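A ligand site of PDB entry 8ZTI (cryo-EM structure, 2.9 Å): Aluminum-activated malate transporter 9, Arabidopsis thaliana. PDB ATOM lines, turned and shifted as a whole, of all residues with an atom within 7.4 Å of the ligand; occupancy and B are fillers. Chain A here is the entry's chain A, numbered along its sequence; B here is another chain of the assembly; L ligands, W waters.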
ATOM      1  N   LEU A 114      17.966  11.943   4.395  1.00  0.00           N
ATOM      2  CA  LEU A 114      17.514  13.313   4.258  1.00  0.00           C
ATOM      3  C   LEU A 114      16.197  13.367   3.492  1.00  0.00           C
ATOM      4  O   LEU A 114      15.862  14.413   2.924  1.00  0.00           O
ATOM      5  CB  LEU A 114      18.575  14.183   3.561  1.00  0.00           C
ATOM      6  CG  LEU A 114      19.500  13.472   2.582  1.00  0.00           C
ATOM      7  CD1 LEU A 114      19.860  14.389   1.425  1.00  0.00           C
ATOM      8  CD2 LEU A 114      20.746  12.978   3.283  1.00  0.00           C
ATOM      9  N   SER A 115      15.464  12.248   3.449  1.00  0.00           N
ATOM     10  CA  SER A 115      14.225  12.104   2.700  1.00  0.00           C
ATOM     11  C   SER A 115      13.337  13.344   2.793  1.00  0.00           C
ATOM     12  O   SER A 115      12.670  13.709   1.811  1.00  0.00           O
ATOM     13  CB  SER A 115      13.458  10.880   3.187  1.00  0.00           C
ATOM     14  OG  SER A 115      12.410  10.525   2.297  1.00  0.00           O
ATOM     15  N   ARG A 116      13.314  13.997   3.945  1.00  0.00           N
ATOM     16  CA  ARG A 116      12.446  15.160   4.133  1.00  0.00           C
ATOM     17  C   ARG A 116      13.167  16.466   3.854  1.00  0.00           C
ATOM     18  O   ARG A 116      12.519  17.484   3.607  1.00  0.00           O
ATOM     19  CB  ARG A 116      11.879  15.188   5.558  1.00  0.00           C
ATOM     20  CG  ARG A 116      12.916  15.009   6.659  1.00  0.00           C
ATOM     21  CD  ARG A 116      12.368  14.194   7.814  1.00  0.00           C
ATOM     22  NE  ARG A 116      12.456  12.756   7.562  1.00  0.00           N
ATOM     23  CZ  ARG A 116      13.594  12.099   7.358  1.00  0.00           C
ATOM     24  NH1 ARG A 116      14.764  12.715   7.369  1.00  0.00           N
ATOM     25  NH2 ARG A 116      13.550  10.787   7.132  1.00  0.00           N
ATOM     26  N   TYR A 117      14.506  16.459   3.881  1.00  0.00           N
ATOM     27  CA  TYR A 117      15.300  17.628   3.549  1.00  0.00           C
ATOM     28  C   TYR A 117      15.710  17.650   2.090  1.00  0.00           C
ATOM     29  O   TYR A 117      16.416  18.572   1.664  1.00  0.00           O
ATOM     30  CB  TYR A 117      16.554  17.682   4.427  1.00  0.00           C
ATOM     31  CG  TYR A 117      16.298  17.661   5.920  1.00  0.00           C
ATOM     32  CD1 TYR A 117      15.009  17.647   6.438  1.00  0.00           C
ATOM     33  CD2 TYR A 117      17.360  17.615   6.817  1.00  0.00           C
ATOM     34  CE1 TYR A 117      14.784  17.616   7.806  1.00  0.00           C
ATOM     35  CE2 TYR A 117      17.148  17.573   8.183  1.00  0.00           C
ATOM     36  CZ  TYR A 117      15.852  17.584   8.669  1.00  0.00           C
ATOM     37  OH  TYR A 117      15.637  17.550  10.029  1.00  0.00           O
ATOM     38  N   SER A 118      15.278  16.659   1.303  1.00  0.00           N
ATOM     39  CA  SER A 118      15.593  16.563  -0.110  1.00  0.00           C
ATOM     40  C   SER A 118      14.530  17.180  -0.997  1.00  0.00           C
ATOM     41  O   SER A 118      14.447  16.840  -2.193  1.00  0.00           O
ATOM     42  CB  SER A 118      15.828  15.099  -0.497  1.00  0.00           C
ATOM     43  OG  SER A 118      16.966  14.578   0.171  1.00  0.00           O
ATOM     44  N   VAL A 119      13.695  18.069  -0.457  1.00  0.00           N
ATOM     45  CA  VAL A 119      12.720  18.802  -1.254  1.00  0.00           C
ATOM     46  C   VAL A 119      13.077  20.272  -1.381  1.00  0.00           C
ATOM     47  O   VAL A 119      12.620  20.924  -2.342  1.00  0.00           O
ATOM     48  CB  VAL A 119      11.301  18.646  -0.677  1.00  0.00           C
ATOM     49  CG1 VAL A 119      10.888  17.183  -0.674  1.00  0.00           C
ATOM     50  CG2 VAL A 119      11.226  19.241   0.721  1.00  0.00           C
ATOM     51  N   TRP A 120      13.873  20.828  -0.462  1.00  0.00           N
ATOM     52  CA  TRP A 120      14.278  22.227  -0.581  1.00  0.00           C
ATOM     53  C   TRP A 120      15.111  22.439  -1.831  1.00  0.00           C
ATOM     54  O   TRP A 120      15.249  23.586  -2.291  1.00  0.00           O
ATOM     55  CB  TRP A 120      15.055  22.640   0.662  1.00  0.00           C
ATOM     56  CG  TRP A 120      14.198  22.786   1.885  1.00  0.00           C
ATOM     57  CD1 TRP A 120      13.849  21.791   2.752  1.00  0.00           C
ATOM     58  CD2 TRP A 120      13.558  23.974   2.349  1.00  0.00           C
ATOM     59  NE1 TRP A 120      13.044  22.301   3.745  1.00  0.00           N
ATOM     60  CE2 TRP A 120      12.856  23.635   3.523  1.00  0.00           C
ATOM     61  CE3 TRP A 120      13.530  25.300   1.910  1.00  0.00           C
ATOM     62  CZ2 TRP A 120      12.117  24.570   4.243  1.00  0.00           C
ATOM     63  CZ3 TRP A 120      12.793  26.228   2.621  1.00  0.00           C
ATOM     64  CH2 TRP A 120      12.099  25.856   3.783  1.00  0.00           C
ATOM     65  N   LEU A 123      12.459  22.511  -4.804  1.00  0.00           N
ATOM     66  CA  LEU A 123      11.512  23.605  -4.715  1.00  0.00           C
ATOM     67  C   LEU A 123      12.182  24.962  -4.927  1.00  0.00           C
ATOM     68  O   LEU A 123      11.487  25.982  -4.970  1.00  0.00           O
ATOM     69  CB  LEU A 123      10.798  23.601  -3.350  1.00  0.00           C
ATOM     70  CG  LEU A 123      10.177  22.278  -2.907  1.00  0.00           C
ATOM     71  CD1 LEU A 123       9.732  22.359  -1.453  1.00  0.00           C
ATOM     72  CD2 LEU A 123       9.011  21.896  -3.808  1.00  0.00           C
ATOM     73  N   TYR A 208      10.785  30.508  10.094  1.00  0.00           N
ATOM     74  CA  TYR A 208      11.138  29.100  10.045  1.00  0.00           C
ATOM     75  C   TYR A 208      12.256  28.783  11.021  1.00  0.00           C
ATOM     76  O   TYR A 208      12.164  27.825  11.799  1.00  0.00           O
ATOM     77  CB  TYR A 208      11.526  28.699   8.627  1.00  0.00           C
ATOM     78  CG  TYR A 208      12.008  27.264   8.517  1.00  0.00           C
ATOM     79  CD1 TYR A 208      11.104  26.216   8.471  1.00  0.00           C
ATOM     80  CD2 TYR A 208      13.372  26.971   8.480  1.00  0.00           C
ATOM     81  CE1 TYR A 208      11.546  24.909   8.374  1.00  0.00           C
ATOM     82  CE2 TYR A 208      13.813  25.665   8.383  1.00  0.00           C
ATOM     83  CZ  TYR A 208      12.895  24.636   8.335  1.00  0.00           C
ATOM     84  OH  TYR A 208      13.333  23.342   8.240  1.00  0.00           O
ATOM     85  N   SER A 212      11.042  26.429  14.086  1.00  0.00           N
ATOM     86  CA  SER A 212      11.372  25.017  13.887  1.00  0.00           C
ATOM     87  C   SER A 212      12.389  24.523  14.902  1.00  0.00           C
ATOM     88  O   SER A 212      12.266  23.408  15.416  1.00  0.00           O
ATOM     89  CB  SER A 212      11.881  24.800  12.453  1.00  0.00           C
ATOM     90  OG  SER A 212      11.709  23.448  12.063  1.00  0.00           O
ATOM     91  N   VAL A 222      20.495  22.851  11.617  1.00  0.00           N
ATOM     92  CA  VAL A 222      19.341  23.076  10.751  1.00  0.00           C
ATOM     93  C   VAL A 222      19.680  24.083   9.651  1.00  0.00           C
ATOM     94  O   VAL A 222      19.281  23.906   8.490  1.00  0.00           O
ATOM     95  CB  VAL A 222      18.125  23.522  11.580  1.00  0.00           C
ATOM     96  CG1 VAL A 222      17.091  24.185  10.677  1.00  0.00           C
ATOM     97  CG2 VAL A 222      17.519  22.340  12.321  1.00  0.00           C
ATOM     98  N   SER A 225      22.245  22.572   7.067  1.00  0.00           N
ATOM     99  CA  SER A 225      21.529  21.602   6.235  1.00  0.00           C
ATOM    100  C   SER A 225      20.593  22.279   5.249  1.00  0.00           C
ATOM    101  O   SER A 225      20.548  21.908   4.068  1.00  0.00           O
ATOM    102  CB  SER A 225      20.754  20.629   7.123  1.00  0.00           C
ATOM    103  OG  SER A 225      19.538  21.208   7.570  1.00  0.00           O
ATOM    104  N   ARG A 226      19.840  23.288   5.701  1.00  0.00           N
ATOM    105  CA  ARG A 226      18.910  23.947   4.791  1.00  0.00           C
ATOM    106  C   ARG A 226      19.619  24.838   3.766  1.00  0.00           C
ATOM    107  O   ARG A 226      18.982  25.252   2.790  1.00  0.00           O
ATOM    108  CB  ARG A 226      17.901  24.778   5.584  1.00  0.00           C
ATOM    109  CG  ARG A 226      16.576  24.102   5.816  1.00  0.00           C
ATOM    110  CD  ARG A 226      16.800  22.701   6.377  1.00  0.00           C
ATOM    111  NE  ARG A 226      15.811  22.337   7.378  1.00  0.00           N
ATOM    112  CZ  ARG A 226      15.948  21.332   8.236  1.00  0.00           C
ATOM    113  NH1 ARG A 226      17.034  20.571   8.236  1.00  0.00           N
ATOM    114  NH2 ARG A 226      14.989  21.094   9.125  1.00  0.00           N
ATOM    115  N   SER B 115       3.821  18.553  15.641  1.00  0.00           N
ATOM    116  CA  SER B 115       5.167  19.092  15.795  1.00  0.00           C
ATOM    117  C   SER B 115       6.018  18.799  14.566  1.00  0.00           C
ATOM    118  O   SER B 115       6.801  19.653  14.126  1.00  0.00           O
ATOM    119  CB  SER B 115       5.828  18.523  17.049  1.00  0.00           C
ATOM    120  OG  SER B 115       5.141  18.943  18.222  1.00  0.00           O
ATOM    121  N   ARG B 116       5.877  17.599  13.996  1.00  0.00           N
ATOM    122  CA  ARG B 116       6.659  17.253  12.820  1.00  0.00           C
ATOM    123  C   ARG B 116       6.390  18.221  11.672  1.00  0.00           C
ATOM    124  O   ARG B 116       7.312  18.588  10.932  1.00  0.00           O
ATOM    125  CB  ARG B 116       6.340  15.822  12.379  1.00  0.00           C
ATOM    126  CG  ARG B 116       7.423  14.807  12.736  1.00  0.00           C
ATOM    127  CD  ARG B 116       7.473  13.663  11.719  1.00  0.00           C
ATOM    128  NE  ARG B 116       8.083  14.076  10.454  1.00  0.00           N
ATOM    129  CZ  ARG B 116       7.433  14.182   9.313  1.00  0.00           C
ATOM    130  NH1 ARG B 116       6.136  13.917   9.216  1.00  0.00           N
ATOM    131  NH2 ARG B 116       8.087  14.557   8.218  1.00  0.00           N
ATOM    132  N   TYR B 117       5.144  18.650  11.527  1.00  0.00           N
ATOM    133  CA  TYR B 117       4.709  19.545  10.457  1.00  0.00           C
ATOM    134  C   TYR B 117       3.894  20.699  11.019  1.00  0.00           C
ATOM    135  O   TYR B 117       2.831  21.052  10.510  1.00  0.00           O
ATOM    136  CB  TYR B 117       3.907  18.739   9.431  1.00  0.00           C
ATOM    137  CG  TYR B 117       3.354  17.450   9.996  1.00  0.00           C
ATOM    138  CD1 TYR B 117       4.122  16.299  10.045  1.00  0.00           C
ATOM    139  CD2 TYR B 117       2.063  17.398  10.516  1.00  0.00           C
ATOM    140  CE1 TYR B 117       3.624  15.118  10.565  1.00  0.00           C
ATOM    141  CE2 TYR B 117       1.554  16.220  11.044  1.00  0.00           C
ATOM    142  CZ  TYR B 117       2.338  15.086  11.058  1.00  0.00           C
ATOM    143  OH  TYR B 117       1.837  13.919  11.581  1.00  0.00           O
ATOM    144  N   SER B 118       4.401  21.320  12.086  1.00  0.00           N
ATOM    145  CA  SER B 118       3.753  22.468  12.702  1.00  0.00           C
ATOM    146  C   SER B 118       4.290  23.790  12.186  1.00  0.00           C
ATOM    147  O   SER B 118       3.762  24.841  12.566  1.00  0.00           O
ATOM    148  CB  SER B 118       3.919  22.410  14.222  1.00  0.00           C
ATOM    149  OG  SER B 118       5.248  22.697  14.606  1.00  0.00           O
ATOM    150  N   VAL B 119       5.321  23.773  11.342  1.00  0.00           N
ATOM    151  CA  VAL B 119       5.863  24.978  10.737  1.00  0.00           C
ATOM    152  C   VAL B 119       5.178  25.209   9.401  1.00  0.00           C
ATOM    153  O   VAL B 119       5.693  25.933   8.544  1.00  0.00           O
ATOM    154  CB  VAL B 119       7.394  24.876  10.575  1.00  0.00           C
ATOM    155  CG1 VAL B 119       7.743  24.176   9.268  1.00  0.00           C
ATOM    156  CG2 VAL B 119       8.023  26.262  10.634  1.00  0.00           C
ATOM    157  N   TRP B 120       4.001  24.603   9.220  1.00  0.00           N
ATOM    158  CA  TRP B 120       3.224  24.758   8.000  1.00  0.00           C
ATOM    159  C   TRP B 120       2.101  25.776   8.132  1.00  0.00           C
ATOM    160  O   TRP B 120       1.537  26.183   7.122  1.00  0.00           O
ATOM    161  CB  TRP B 120       2.639  23.409   7.586  1.00  0.00           C
ATOM    162  CG  TRP B 120       3.557  22.571   6.747  1.00  0.00           C
ATOM    163  CD1 TRP B 120       4.662  21.902   7.181  1.00  0.00           C
ATOM    164  CD2 TRP B 120       3.450  22.309   5.343  1.00  0.00           C
ATOM    165  NE1 TRP B 120       5.255  21.242   6.129  1.00  0.00           N
ATOM    166  CE2 TRP B 120       4.533  21.478   4.996  1.00  0.00           C
ATOM    167  CE3 TRP B 120       2.542  22.693   4.349  1.00  0.00           C
ATOM    168  CZ2 TRP B 120       4.731  21.022   3.690  1.00  0.00           C
ATOM    169  CZ3 TRP B 120       2.749  22.244   3.064  1.00  0.00           C
ATOM    170  CH2 TRP B 120       3.831  21.422   2.748  1.00  0.00           C
ATOM    171  N   LEU B 123       3.416  29.782   7.865  1.00  0.00           N
ATOM    172  CA  LEU B 123       3.874  30.134   6.522  1.00  0.00           C
ATOM    173  C   LEU B 123       2.716  30.317   5.550  1.00  0.00           C
ATOM    174  O   LEU B 123       2.951  30.633   4.386  1.00  0.00           O
ATOM    175  CB  LEU B 123       4.834  29.062   5.983  1.00  0.00           C
ATOM    176  CG  LEU B 123       5.862  28.475   6.955  1.00  0.00           C
ATOM    177  CD1 LEU B 123       6.644  27.361   6.272  1.00  0.00           C
ATOM    178  CD2 LEU B 123       6.791  29.552   7.468  1.00  0.00           C
ATOM    179  N   TYR B 208       5.984  18.459  -4.525  1.00  0.00           N
ATOM    180  CA  TYR B 208       6.084  18.059  -3.128  1.00  0.00           C
ATOM    181  C   TYR B 208       5.379  16.721  -2.897  1.00  0.00           C
ATOM    182  O   TYR B 208       5.949  15.812  -2.294  1.00  0.00           O
ATOM    183  CB  TYR B 208       5.489  19.146  -2.223  1.00  0.00           C
ATOM    184  CG  TYR B 208       5.447  18.741  -0.769  1.00  0.00           C
ATOM    185  CD1 TYR B 208       6.537  18.961   0.064  1.00  0.00           C
ATOM    186  CD2 TYR B 208       4.314  18.157  -0.227  1.00  0.00           C
ATOM    187  CE1 TYR B 208       6.493  18.595   1.402  1.00  0.00           C
ATOM    188  CE2 TYR B 208       4.261  17.789   1.112  1.00  0.00           C
ATOM    189  CZ  TYR B 208       5.358  18.015   1.917  1.00  0.00           C
ATOM    190  OH  TYR B 208       5.314  17.652   3.241  1.00  0.00           O
ATOM    191  N   SER B 212       7.748  13.561  -1.883  1.00  0.00           N
ATOM    192  CA  SER B 212       7.693  13.254  -0.464  1.00  0.00           C
ATOM    193  C   SER B 212       7.324  11.807  -0.168  1.00  0.00           C
ATOM    194  O   SER B 212       8.147  11.034   0.325  1.00  0.00           O
ATOM    195  CB  SER B 212       6.716  14.194   0.242  1.00  0.00           C
ATOM    196  OG  SER B 212       6.608  13.889   1.615  1.00  0.00           O
ATOM    197  N   ARG B 226      -1.291  18.126   5.859  1.00  0.00           N
ATOM    198  CA  ARG B 226      -0.860  19.477   5.518  1.00  0.00           C
ATOM    199  C   ARG B 226      -2.051  20.335   5.109  1.00  0.00           C
ATOM    200  O   ARG B 226      -2.098  21.521   5.437  1.00  0.00           O
ATOM    201  CB  ARG B 226       0.202  19.432   4.425  1.00  0.00           C
ATOM    202  CG  ARG B 226       1.591  19.099   4.969  1.00  0.00           C
ATOM    203  CD  ARG B 226       2.034  17.709   4.559  1.00  0.00           C
ATOM    204  NE  ARG B 226       3.360  17.374   5.070  1.00  0.00           N
ATOM    205  CZ  ARG B 226       3.579  16.464   6.008  1.00  0.00           C
ATOM    206  NH1 ARG B 226       2.598  15.761   6.546  1.00  0.00           N
ATOM    207  NH2 ARG B 226       4.834  16.246   6.411  1.00  0.00           N
HETATM  208  C1  LIG L   1       9.296  19.755   6.030  1.00  0.00           C
HETATM  209  O1  LIG L   1       9.930  19.740   4.953  1.00  0.00           O
HETATM  210  O2  LIG L   1       8.219  19.106   6.131  1.00  0.00           O
HETATM  211  C2  LIG L   1       9.815  20.556   7.229  1.00  0.00           C
HETATM  212  O3  LIG L   1       8.942  21.619   7.489  1.00  0.00           O
HETATM  213  C3  LIG L   1      11.202  21.089   6.923  1.00  0.00           C
HETATM  214  C4  LIG L   1      12.195  19.928   6.813  1.00  0.00           C
HETATM  215  O4  LIG L   1      11.853  18.761   7.147  1.00  0.00           O
HETATM  216  O5  LIG L   1      13.358  20.134   6.388  1.00  0.00           O
HETATM  217  O   HOH W   1       7.453  23.857   6.213  1.00  0.00           O
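O5 of the ligand lies within salt-bridge range of NH2 of Arg 226 of chain A (3.3 Å).
The indole nitrogen (NE1) of Trp 120 of chain A is in hydrogen-bond range of an oxygen (O5) of the ligand (3.4 Å).
Water W1 lies within hydrogen-bond range of O3 of the ligand (3.0 Å) and NE1 of Trp 120 of chain B (3.4 Å).
Merely in contact with the ligand: Arg 116 of chain A (3.7 Å), Tyr 117 of chain A (3.0 Å), Tyr 208 of chain A (3.4 Å), Val 119 of chain B (3.3 Å) and Trp 120 of chain B (3.7 Å).
Seven residues have an atom within 4 Å of the ligand: Arg 116 of chain A, Tyr 117 of chain A, Trp 120 of chain A, Tyr 208 of chain A, Arg 226 of chain A, Val 119 of chain B and Trp 120 of chain B.
The nearest printed residue that does not touch the ligand is Tyr 208 of chain B (4.3 Å).
The guanidinium group of Arg 226 of chain A lies within hydrogen-bond range of the side-chain hydroxyl of Tyr 208 of chain A, at 2.8 Å.
The guanidinium group (NH1) of Arg 226 of chain A sits at hydrogen-bond distance from the side-chain hydroxyl (OG) of Ser 225 (2.7 Å).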
